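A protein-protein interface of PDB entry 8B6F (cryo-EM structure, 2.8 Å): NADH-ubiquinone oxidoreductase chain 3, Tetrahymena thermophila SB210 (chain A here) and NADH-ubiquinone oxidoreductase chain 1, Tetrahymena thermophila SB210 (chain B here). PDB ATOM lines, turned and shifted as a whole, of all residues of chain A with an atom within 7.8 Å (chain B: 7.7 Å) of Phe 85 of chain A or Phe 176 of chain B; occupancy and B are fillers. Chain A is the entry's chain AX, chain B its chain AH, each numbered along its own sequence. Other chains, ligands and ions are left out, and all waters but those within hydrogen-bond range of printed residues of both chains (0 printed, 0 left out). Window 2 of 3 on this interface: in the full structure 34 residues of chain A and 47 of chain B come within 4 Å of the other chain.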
ATOM      1  N   PHE A  79      20.814  -7.281 -19.620  1.00  0.00           N
ATOM      2  CA  PHE A  79      19.668  -7.894 -18.953  1.00  0.00           C
ATOM      3  C   PHE A  79      18.496  -8.145 -19.890  1.00  0.00           C
ATOM      4  O   PHE A  79      17.958  -9.266 -19.879  1.00  0.00           O
ATOM      5  CB  PHE A  79      19.250  -7.028 -17.762  1.00  0.00           C
ATOM      6  CG  PHE A  79      20.035  -7.304 -16.513  1.00  0.00           C
ATOM      7  CD1 PHE A  79      21.255  -6.689 -16.299  1.00  0.00           C
ATOM      8  CD2 PHE A  79      19.561  -8.187 -15.560  1.00  0.00           C
ATOM      9  CE1 PHE A  79      21.984  -6.940 -15.154  1.00  0.00           C
ATOM     10  CE2 PHE A  79      20.286  -8.445 -14.412  1.00  0.00           C
ATOM     11  CZ  PHE A  79      21.498  -7.822 -14.209  1.00  0.00           C
ATOM     12  N   PRO A  80      18.044  -7.188 -20.707  1.00  0.00           N
ATOM     13  CA  PRO A  80      16.854  -7.466 -21.534  1.00  0.00           C
ATOM     14  C   PRO A  80      17.026  -8.642 -22.482  1.00  0.00           C
ATOM     15  O   PRO A  80      16.084  -9.422 -22.664  1.00  0.00           O
ATOM     16  CB  PRO A  80      16.633  -6.145 -22.287  1.00  0.00           C
ATOM     17  CG  PRO A  80      17.920  -5.423 -22.209  1.00  0.00           C
ATOM     18  CD  PRO A  80      18.543  -5.817 -20.911  1.00  0.00           C
ATOM     19  N   VAL A  81      18.198  -8.793 -23.101  1.00  0.00           N
ATOM     20  CA  VAL A  81      18.393  -9.899 -24.034  1.00  0.00           C
ATOM     21  C   VAL A  81      18.410 -11.230 -23.290  1.00  0.00           C
ATOM     22  O   VAL A  81      17.887 -12.236 -23.784  1.00  0.00           O
ATOM     23  CB  VAL A  81      19.675  -9.690 -24.863  1.00  0.00           C
ATOM     24  CG1 VAL A  81      20.893  -9.522 -23.968  1.00  0.00           C
ATOM     25  CG2 VAL A  81      19.882 -10.845 -25.832  1.00  0.00           C
ATOM     26  N   LEU A  82      19.006 -11.261 -22.097  1.00  0.00           N
ATOM     27  CA  LEU A  82      18.986 -12.480 -21.295  1.00  0.00           C
ATOM     28  C   LEU A  82      17.567 -12.835 -20.873  1.00  0.00           C
ATOM     29  O   LEU A  82      17.178 -14.008 -20.900  1.00  0.00           O
ATOM     30  CB  LEU A  82      19.882 -12.313 -20.070  1.00  0.00           C
ATOM     31  CG  LEU A  82      21.357 -12.042 -20.368  1.00  0.00           C
ATOM     32  CD1 LEU A  82      22.081 -11.627 -19.104  1.00  0.00           C
ATOM     33  CD2 LEU A  82      22.022 -13.256 -20.992  1.00  0.00           C
ATOM     34  N   PHE A  83      16.779 -11.834 -20.480  1.00  0.00           N
ATOM     35  CA  PHE A  83      15.408 -12.093 -20.056  1.00  0.00           C
ATOM     36  C   PHE A  83      14.562 -12.622 -21.206  1.00  0.00           C
ATOM     37  O   PHE A  83      13.760 -13.545 -21.022  1.00  0.00           O
ATOM     38  CB  PHE A  83      14.790 -10.821 -19.477  1.00  0.00           C
ATOM     39  CG  PHE A  83      15.021 -10.656 -18.005  1.00  0.00           C
ATOM     40  CD1 PHE A  83      16.266 -10.303 -17.518  1.00  0.00           C
ATOM     41  CD2 PHE A  83      13.986 -10.846 -17.108  1.00  0.00           C
ATOM     42  CE1 PHE A  83      16.475 -10.147 -16.162  1.00  0.00           C
ATOM     43  CE2 PHE A  83      14.189 -10.692 -15.753  1.00  0.00           C
ATOM     44  CZ  PHE A  83      15.435 -10.341 -15.278  1.00  0.00           C
ATOM     45  N   ASN A  84      14.720 -12.051 -22.396  1.00  0.00           N
ATOM     46  CA  ASN A  84      13.916 -12.408 -23.560  1.00  0.00           C
ATOM     47  C   ASN A  84      14.740 -13.151 -24.606  1.00  0.00           C
ATOM     48  O   ASN A  84      14.561 -12.960 -25.810  1.00  0.00           O
ATOM     49  CB  ASN A  84      13.286 -11.163 -24.176  1.00  0.00           C
ATOM     50  CG  ASN A  84      12.356 -10.449 -23.220  1.00  0.00           C
ATOM     51  OD1 ASN A  84      11.231 -10.887 -22.989  1.00  0.00           O
ATOM     52  ND2 ASN A  84      12.818  -9.336 -22.667  1.00  0.00           N
ATOM     53  N   PHE A  85      15.662 -14.006 -24.160  1.00  0.00           N
ATOM     54  CA  PHE A  85      16.463 -14.776 -25.101  1.00  0.00           C
ATOM     55  C   PHE A  85      15.641 -15.819 -25.846  1.00  0.00           C
ATOM     56  O   PHE A  85      16.094 -16.324 -26.876  1.00  0.00           O
ATOM     57  CB  PHE A  85      17.629 -15.453 -24.386  1.00  0.00           C
ATOM     58  CG  PHE A  85      18.683 -15.972 -25.318  1.00  0.00           C
ATOM     59  CD1 PHE A  85      19.668 -15.132 -25.810  1.00  0.00           C
ATOM     60  CD2 PHE A  85      18.694 -17.303 -25.698  1.00  0.00           C
ATOM     61  CE1 PHE A  85      20.636 -15.608 -26.671  1.00  0.00           C
ATOM     62  CE2 PHE A  85      19.660 -17.785 -26.557  1.00  0.00           C
ATOM     63  CZ  PHE A  85      20.634 -16.937 -27.042  1.00  0.00           C
ATOM     64  N   SER A  86      14.450 -16.159 -25.350  1.00  0.00           N
ATOM     65  CA  SER A  86      13.560 -17.028 -26.108  1.00  0.00           C
ATOM     66  C   SER A  86      13.061 -16.357 -27.380  1.00  0.00           C
ATOM     67  O   SER A  86      12.644 -17.053 -28.310  1.00  0.00           O
ATOM     68  CB  SER A  86      12.371 -17.454 -25.246  1.00  0.00           C
ATOM     69  OG  SER A  86      11.589 -16.336 -24.863  1.00  0.00           O
ATOM     70  N   MET A  87      13.098 -15.028 -27.439  1.00  0.00           N
ATOM     71  CA  MET A  87      12.701 -14.269 -28.616  1.00  0.00           C
ATOM     72  C   MET A  87      13.874 -13.953 -29.532  1.00  0.00           C
ATOM     73  O   MET A  87      13.708 -13.190 -30.489  1.00  0.00           O
ATOM     74  CB  MET A  87      12.024 -12.960 -28.198  1.00  0.00           C
ATOM     75  CG  MET A  87      10.882 -13.123 -27.206  1.00  0.00           C
ATOM     76  SD  MET A  87      10.213 -11.533 -26.676  1.00  0.00           S
ATOM     77  CE  MET A  87       9.009 -12.056 -25.462  1.00  0.00           C
ATOM     78  N   PHE A  88      15.052 -14.510 -29.260  1.00  0.00           N
ATOM     79  CA  PHE A  88      16.248 -14.115 -29.990  1.00  0.00           C
ATOM     80  C   PHE A  88      16.097 -14.414 -31.475  1.00  0.00           C
ATOM     81  O   PHE A  88      15.477 -15.403 -31.872  1.00  0.00           O
ATOM     82  CB  PHE A  88      17.473 -14.841 -29.434  1.00  0.00           C
ATOM     83  CG  PHE A  88      17.697 -16.200 -30.035  1.00  0.00           C
ATOM     84  CD1 PHE A  88      17.012 -17.305 -29.561  1.00  0.00           C
ATOM     85  CD2 PHE A  88      18.608 -16.373 -31.065  1.00  0.00           C
ATOM     86  CE1 PHE A  88      17.219 -18.555 -30.110  1.00  0.00           C
ATOM     87  CE2 PHE A  88      18.821 -17.620 -31.618  1.00  0.00           C
ATOM     88  CZ  PHE A  88      18.125 -18.712 -31.139  1.00  0.00           C
ATOM     89  N   SER A  89      16.665 -13.536 -32.299  1.00  0.00           N
ATOM     90  CA  SER A  89      16.745 -13.754 -33.736  1.00  0.00           C
ATOM     91  C   SER A  89      18.185 -13.555 -34.187  1.00  0.00           C
ATOM     92  O   SER A  89      19.080 -13.391 -33.353  1.00  0.00           O
ATOM     93  CB  SER A  89      15.803 -12.811 -34.485  1.00  0.00           C
ATOM     94  OG  SER A  89      16.128 -11.456 -34.234  1.00  0.00           O
ATOM     95  N   GLU A  92      19.498 -10.052 -32.985  1.00  0.00           N
ATOM     96  CA  GLU A  92      19.687  -9.964 -31.542  1.00  0.00           C
ATOM     97  C   GLU A  92      20.866 -10.813 -31.090  1.00  0.00           C
ATOM     98  O   GLU A  92      21.667 -10.384 -30.252  1.00  0.00           O
ATOM     99  CB  GLU A  92      18.411 -10.388 -30.819  1.00  0.00           C
ATOM    100  CG  GLU A  92      17.190  -9.586 -31.231  1.00  0.00           C
ATOM    101  CD  GLU A  92      15.955  -9.962 -30.442  1.00  0.00           C
ATOM    102  OE1 GLU A  92      16.092 -10.699 -29.444  1.00  0.00           O
ATOM    103  OE2 GLU A  92      14.848  -9.526 -30.821  1.00  0.00           O
ATOM    104  N   LEU A  93      20.987 -12.023 -31.632  1.00  0.00           N
ATOM    105  CA  LEU A  93      22.113 -12.880 -31.281  1.00  0.00           C
ATOM    106  C   LEU A  93      23.433 -12.232 -31.681  1.00  0.00           C
ATOM    107  O   LEU A  93      24.394 -12.222 -30.906  1.00  0.00           O
ATOM    108  CB  LEU A  93      21.952 -14.243 -31.953  1.00  0.00           C
ATOM    109  CG  LEU A  93      22.871 -15.358 -31.456  1.00  0.00           C
ATOM    110  CD1 LEU A  93      22.528 -15.736 -30.023  1.00  0.00           C
ATOM    111  CD2 LEU A  93      22.785 -16.566 -32.369  1.00  0.00           C
ATOM    112  N   ALA A  96      24.204  -9.312 -29.274  1.00  0.00           N
ATOM    113  CA  ALA A  96      24.620  -9.757 -27.949  1.00  0.00           C
ATOM    114  C   ALA A  96      26.062 -10.248 -27.969  1.00  0.00           C
ATOM    115  O   ALA A  96      26.865  -9.888 -27.101  1.00  0.00           O
ATOM    116  CB  ALA A  96      23.684 -10.857 -27.451  1.00  0.00           C
ATOM    117  N   PHE A  97      26.409 -11.077 -28.955  1.00  0.00           N
ATOM    118  CA  PHE A  97      27.779 -11.569 -29.051  1.00  0.00           C
ATOM    119  C   PHE A  97      28.749 -10.430 -29.327  1.00  0.00           C
ATOM    120  O   PHE A  97      29.864 -10.408 -28.793  1.00  0.00           O
ATOM    121  CB  PHE A  97      27.875 -12.639 -30.139  1.00  0.00           C
ATOM    122  CG  PHE A  97      27.140 -13.915 -29.815  1.00  0.00           C
ATOM    123  CD1 PHE A  97      26.710 -14.192 -28.524  1.00  0.00           C
ATOM    124  CD2 PHE A  97      26.886 -14.843 -30.808  1.00  0.00           C
ATOM    125  CE1 PHE A  97      26.039 -15.366 -28.237  1.00  0.00           C
ATOM    126  CE2 PHE A  97      26.216 -16.019 -30.526  1.00  0.00           C
ATOM    127  CZ  PHE A  97      25.794 -16.280 -29.240  1.00  0.00           C
ATOM    128  N   LEU B 170      27.274 -13.702 -11.677  1.00  0.00           N
ATOM    129  CA  LEU B 170      26.512 -14.867 -11.237  1.00  0.00           C
ATOM    130  C   LEU B 170      25.028 -14.677 -11.518  1.00  0.00           C
ATOM    131  O   LEU B 170      24.358 -15.592 -12.011  1.00  0.00           O
ATOM    132  CB  LEU B 170      26.751 -15.124  -9.749  1.00  0.00           C
ATOM    133  CG  LEU B 170      25.916 -16.244  -9.120  1.00  0.00           C
ATOM    134  CD1 LEU B 170      26.074 -17.549  -9.885  1.00  0.00           C
ATOM    135  CD2 LEU B 170      26.295 -16.438  -7.663  1.00  0.00           C
ATOM    136  N   VAL B 171      24.497 -13.495 -11.208  1.00  0.00           N
ATOM    137  CA  VAL B 171      23.081 -13.230 -11.439  1.00  0.00           C
ATOM    138  C   VAL B 171      22.775 -13.213 -12.929  1.00  0.00           C
ATOM    139  O   VAL B 171      21.718 -13.681 -13.363  1.00  0.00           O
ATOM    140  CB  VAL B 171      22.668 -11.912 -10.760  1.00  0.00           C
ATOM    141  CG1 VAL B 171      21.292 -11.466 -11.236  1.00  0.00           C
ATOM    142  CG2 VAL B 171      22.674 -12.074  -9.251  1.00  0.00           C
ATOM    143  N   ILE B 172      23.694 -12.686 -13.737  1.00  0.00           N
ATOM    144  CA  ILE B 172      23.484 -12.675 -15.181  1.00  0.00           C
ATOM    145  C   ILE B 172      23.397 -14.096 -15.717  1.00  0.00           C
ATOM    146  O   ILE B 172      22.545 -14.406 -16.558  1.00  0.00           O
ATOM    147  CB  ILE B 172      24.597 -11.861 -15.870  1.00  0.00           C
ATOM    148  CG1 ILE B 172      24.149 -10.406 -16.031  1.00  0.00           C
ATOM    149  CG2 ILE B 172      24.995 -12.481 -17.211  1.00  0.00           C
ATOM    150  CD1 ILE B 172      25.232  -9.474 -16.510  1.00  0.00           C
ATOM    151  N   ASN B 173      24.278 -14.981 -15.251  1.00  0.00           N
ATOM    152  CA  ASN B 173      24.208 -16.372 -15.686  1.00  0.00           C
ATOM    153  C   ASN B 173      22.924 -17.039 -15.206  1.00  0.00           C
ATOM    154  O   ASN B 173      22.337 -17.853 -15.927  1.00  0.00           O
ATOM    155  CB  ASN B 173      25.432 -17.136 -15.186  1.00  0.00           C
ATOM    156  CG  ASN B 173      26.705 -16.718 -15.891  1.00  0.00           C
ATOM    157  OD1 ASN B 173      26.817 -15.596 -16.379  1.00  0.00           O
ATOM    158  ND2 ASN B 173      27.674 -17.623 -15.950  1.00  0.00           N
ATOM    159  N   LEU B 174      22.475 -16.713 -13.992  1.00  0.00           N
ATOM    160  CA  LEU B 174      21.297 -17.374 -13.438  1.00  0.00           C
ATOM    161  C   LEU B 174      20.018 -16.917 -14.132  1.00  0.00           C
ATOM    162  O   LEU B 174      19.167 -17.740 -14.485  1.00  0.00           O
ATOM    163  CB  LEU B 174      21.212 -17.117 -11.933  1.00  0.00           C
ATOM    164  CG  LEU B 174      22.262 -17.825 -11.075  1.00  0.00           C
ATOM    165  CD1 LEU B 174      22.170 -17.362  -9.632  1.00  0.00           C
ATOM    166  CD2 LEU B 174      22.116 -19.335 -11.159  1.00  0.00           C
ATOM    167  N   ILE B 175      19.861 -15.607 -14.338  1.00  0.00           N
ATOM    168  CA  ILE B 175      18.640 -15.096 -14.952  1.00  0.00           C
ATOM    169  C   ILE B 175      18.478 -15.612 -16.371  1.00  0.00           C
ATOM    170  O   ILE B 175      17.362 -15.628 -16.901  1.00  0.00           O
ATOM    171  CB  ILE B 175      18.617 -13.554 -14.939  1.00  0.00           C
ATOM    172  CG1 ILE B 175      19.793 -13.003 -15.755  1.00  0.00           C
ATOM    173  CG2 ILE B 175      18.608 -13.046 -13.500  1.00  0.00           C
ATOM    174  CD1 ILE B 175      19.907 -11.497 -15.752  1.00  0.00           C
ATOM    175  N   PHE B 176      19.574 -16.019 -17.009  1.00  0.00           N
ATOM    176  CA  PHE B 176      19.494 -16.563 -18.356  1.00  0.00           C
ATOM    177  C   PHE B 176      18.610 -17.800 -18.428  1.00  0.00           C
ATOM    178  O   PHE B 176      18.117 -18.133 -19.512  1.00  0.00           O
ATOM    179  CB  PHE B 176      20.902 -16.880 -18.859  1.00  0.00           C
ATOM    180  CG  PHE B 176      20.928 -17.492 -20.221  1.00  0.00           C
ATOM    181  CD1 PHE B 176      20.406 -16.815 -21.308  1.00  0.00           C
ATOM    182  CD2 PHE B 176      21.501 -18.735 -20.419  1.00  0.00           C
ATOM    183  CE1 PHE B 176      20.432 -17.375 -22.562  1.00  0.00           C
ATOM    184  CE2 PHE B 176      21.534 -19.300 -21.672  1.00  0.00           C
ATOM    185  CZ  PHE B 176      21.001 -18.619 -22.748  1.00  0.00           C
ATOM    186  N   ILE B 177      18.395 -18.483 -17.306  1.00  0.00           N
ATOM    187  CA  ILE B 177      17.535 -19.659 -17.261  1.00  0.00           C
ATOM    188  C   ILE B 177      16.178 -19.266 -16.694  1.00  0.00           C
ATOM    189  O   ILE B 177      15.141 -19.471 -17.335  1.00  0.00           O
ATOM    190  CB  ILE B 177      18.178 -20.790 -16.433  1.00  0.00           C
ATOM    191  CG1 ILE B 177      19.285 -21.496 -17.225  1.00  0.00           C
ATOM    192  CG2 ILE B 177      17.135 -21.807 -15.984  1.00  0.00           C
ATOM    193  CD1 ILE B 177      20.511 -20.653 -17.508  1.00  0.00           C
ATOM    194  N   SER B 178      16.174 -18.704 -15.485  1.00  0.00           N
ATOM    195  CA  SER B 178      14.916 -18.367 -14.825  1.00  0.00           C
ATOM    196  C   SER B 178      14.142 -17.312 -15.604  1.00  0.00           C
ATOM    197  O   SER B 178      12.917 -17.407 -15.739  1.00  0.00           O
ATOM    198  CB  SER B 178      15.186 -17.881 -13.404  1.00  0.00           C
ATOM    199  OG  SER B 178      15.962 -16.697 -13.425  1.00  0.00           O
ATOM    200  N   GLU B 179      14.837 -16.292 -16.110  1.00  0.00           N
ATOM    201  CA  GLU B 179      14.236 -15.169 -16.825  1.00  0.00           C
ATOM    202  C   GLU B 179      13.468 -14.230 -15.901  1.00  0.00           C
ATOM    203  O   GLU B 179      12.574 -13.511 -16.354  1.00  0.00           O
ATOM    204  CB  GLU B 179      13.308 -15.652 -17.947  1.00  0.00           C
ATOM    205  CG  GLU B 179      13.945 -16.659 -18.892  1.00  0.00           C
ATOM    206  CD  GLU B 179      12.981 -17.142 -19.959  1.00  0.00           C
ATOM    207  OE1 GLU B 179      11.856 -16.606 -20.029  1.00  0.00           O
ATOM    208  OE2 GLU B 179      13.345 -18.060 -20.722  1.00  0.00           O
ATOM    209  N   SER B 180      13.790 -14.224 -14.610  1.00  0.00           N
ATOM    210  CA  SER B 180      13.137 -13.328 -13.667  1.00  0.00           C
ATOM    211  C   SER B 180      14.037 -13.139 -12.458  1.00  0.00           C
ATOM    212  O   SER B 180      14.944 -13.935 -12.205  1.00  0.00           O
ATOM    213  CB  SER B 180      11.791 -13.874 -13.207  1.00  0.00           C
ATOM    214  OG  SER B 180      12.010 -15.054 -12.465  1.00  0.00           O
ATOM    215  N   PHE B 186      12.911 -19.978  -9.969  1.00  0.00           N
ATOM    216  CA  PHE B 186      14.032 -20.904 -10.075  1.00  0.00           C
ATOM    217  C   PHE B 186      13.610 -22.324  -9.718  1.00  0.00           C
ATOM    218  O   PHE B 186      14.052 -23.284 -10.358  1.00  0.00           O
ATOM    219  CB  PHE B 186      15.181 -20.452  -9.174  1.00  0.00           C
ATOM    220  CG  PHE B 186      15.789 -19.146  -9.581  1.00  0.00           C
ATOM    221  CD1 PHE B 186      15.248 -17.948  -9.151  1.00  0.00           C
ATOM    222  CD2 PHE B 186      16.914 -19.118 -10.388  1.00  0.00           C
ATOM    223  CE1 PHE B 186      15.813 -16.743  -9.525  1.00  0.00           C
ATOM    224  CE2 PHE B 186      17.484 -17.920 -10.765  1.00  0.00           C
ATOM    225  CZ  PHE B 186      16.933 -16.731 -10.332  1.00  0.00           C
ATOM    226  N   LEU B 195      19.790 -26.644 -10.342  1.00  0.00           N
ATOM    227  CA  LEU B 195      20.503 -25.799 -11.291  1.00  0.00           C
ATOM    228  C   LEU B 195      22.011 -25.850 -11.106  1.00  0.00           C
ATOM    229  O   LEU B 195      22.740 -25.389 -11.989  1.00  0.00           O
ATOM    230  CB  LEU B 195      20.024 -24.352 -11.169  1.00  0.00           C
ATOM    231  CG  LEU B 195      19.641 -23.664 -12.479  1.00  0.00           C
ATOM    232  CD1 LEU B 195      18.403 -24.311 -13.080  1.00  0.00           C
ATOM    233  CD2 LEU B 195      19.417 -22.177 -12.256  1.00  0.00           C
ATOM    234  N   ILE B 198      24.194 -27.540 -14.022  1.00  0.00           N
ATOM    235  CA  ILE B 198      24.640 -26.745 -15.162  1.00  0.00           C
ATOM    236  C   ILE B 198      25.935 -26.023 -14.820  1.00  0.00           C
ATOM    237  O   ILE B 198      26.830 -25.886 -15.663  1.00  0.00           O
ATOM    238  CB  ILE B 198      23.538 -25.759 -15.591  1.00  0.00           C
ATOM    239  CG1 ILE B 198      22.307 -26.528 -16.072  1.00  0.00           C
ATOM    240  CG2 ILE B 198      24.046 -24.824 -16.687  1.00  0.00           C
ATOM    241  CD1 ILE B 198      21.095 -25.660 -16.309  1.00  0.00           C
ATOM    242  N   PHE B 199      26.059 -25.556 -13.580  1.00  0.00           N
ATOM    243  CA  PHE B 199      27.205 -24.778 -13.135  1.00  0.00           C
ATOM    244  C   PHE B 199      28.255 -25.629 -12.438  1.00  0.00           C
ATOM    245  O   PHE B 199      29.143 -25.080 -11.778  1.00  0.00           O
ATOM    246  CB  PHE B 199      26.744 -23.656 -12.205  1.00  0.00           C
ATOM    247  CG  PHE B 199      25.880 -22.634 -12.879  1.00  0.00           C
ATOM    248  CD1 PHE B 199      24.534 -22.877 -13.090  1.00  0.00           C
ATOM    249  CD2 PHE B 199      26.414 -21.430 -13.303  1.00  0.00           C
ATOM    250  CE1 PHE B 199      23.736 -21.937 -13.712  1.00  0.00           C
ATOM    251  CE2 PHE B 199      25.624 -20.487 -13.926  1.00  0.00           C
ATOM    252  CZ  PHE B 199      24.282 -20.740 -14.132  1.00  0.00           C
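OG of Ser 178 of chain B is in hydrogen-bond range of O of Ser 180 of chain B (3.2 Å).
Phe 79 of chain A touches Ile 175 of chain B (CD2 to CD1, 3.3 Å). Leu 82 of chain A touches Ile 172 of chain B (CD1 to CG2, 3.6 Å). Ile 175 of chain B touches Leu 82 of chain A. Phe 176 of chain B touches Leu 82 of chain A. Phe 83 of chain A touches Ile 175 of chain B (CE1 to CD1, 3.7 Å). Phe 83 of chain A touches Glu 179 of chain B (CD2 to O, 3.1 Å). CE2 of Phe 83 of chain A touches CA of Ser 180 of chain B (3.5 Å). Phe 176 of chain B touches Phe 85 of chain A (CE1 to CG, 3.6 Å).
Of the printed residues of chain B, Leu 82 of chain A touches Ile 172 (3.6 Å), Ile 175 (3.997 Å) and Phe 176 (3.9 Å). Of the printed residues of chain B, Phe 83 of chain A touches Ile 175, Glu 179 and Ser 180. Phe 85 of chain A touches just one residue of chain B: Phe 176. Of the printed residues of chain A, Ile 172 of chain B touches Leu 82. Of the printed residues of chain A, Ile 175 of chain B touches Phe 79 (3.3 Å), Leu 82 (3.997 Å) and Phe 83 (3.7 Å). Phe 176 of chain B touches two residues of chain A. Of the printed residues of chain A, Ser 180 of chain B touches Phe 83 (3.5 Å). The nearest residue of chain B that does not touch Phe 85 of chain A is Glu 179 of chain B (5.8 Å). The nearest printed residue of chain A that does not touch Ser 180 of chain B is Leu 82 of chain A (7.1 Å).
Of the 15 printed residues of chain A, 4 touch a printed residue of chain B. Among the printed residues, 8 pairs touch across the chains. Among the printed residues, no Asp or Glu carboxylate lies within 4 Å of a Lys or Arg side-chain nitrogen of the other chain.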
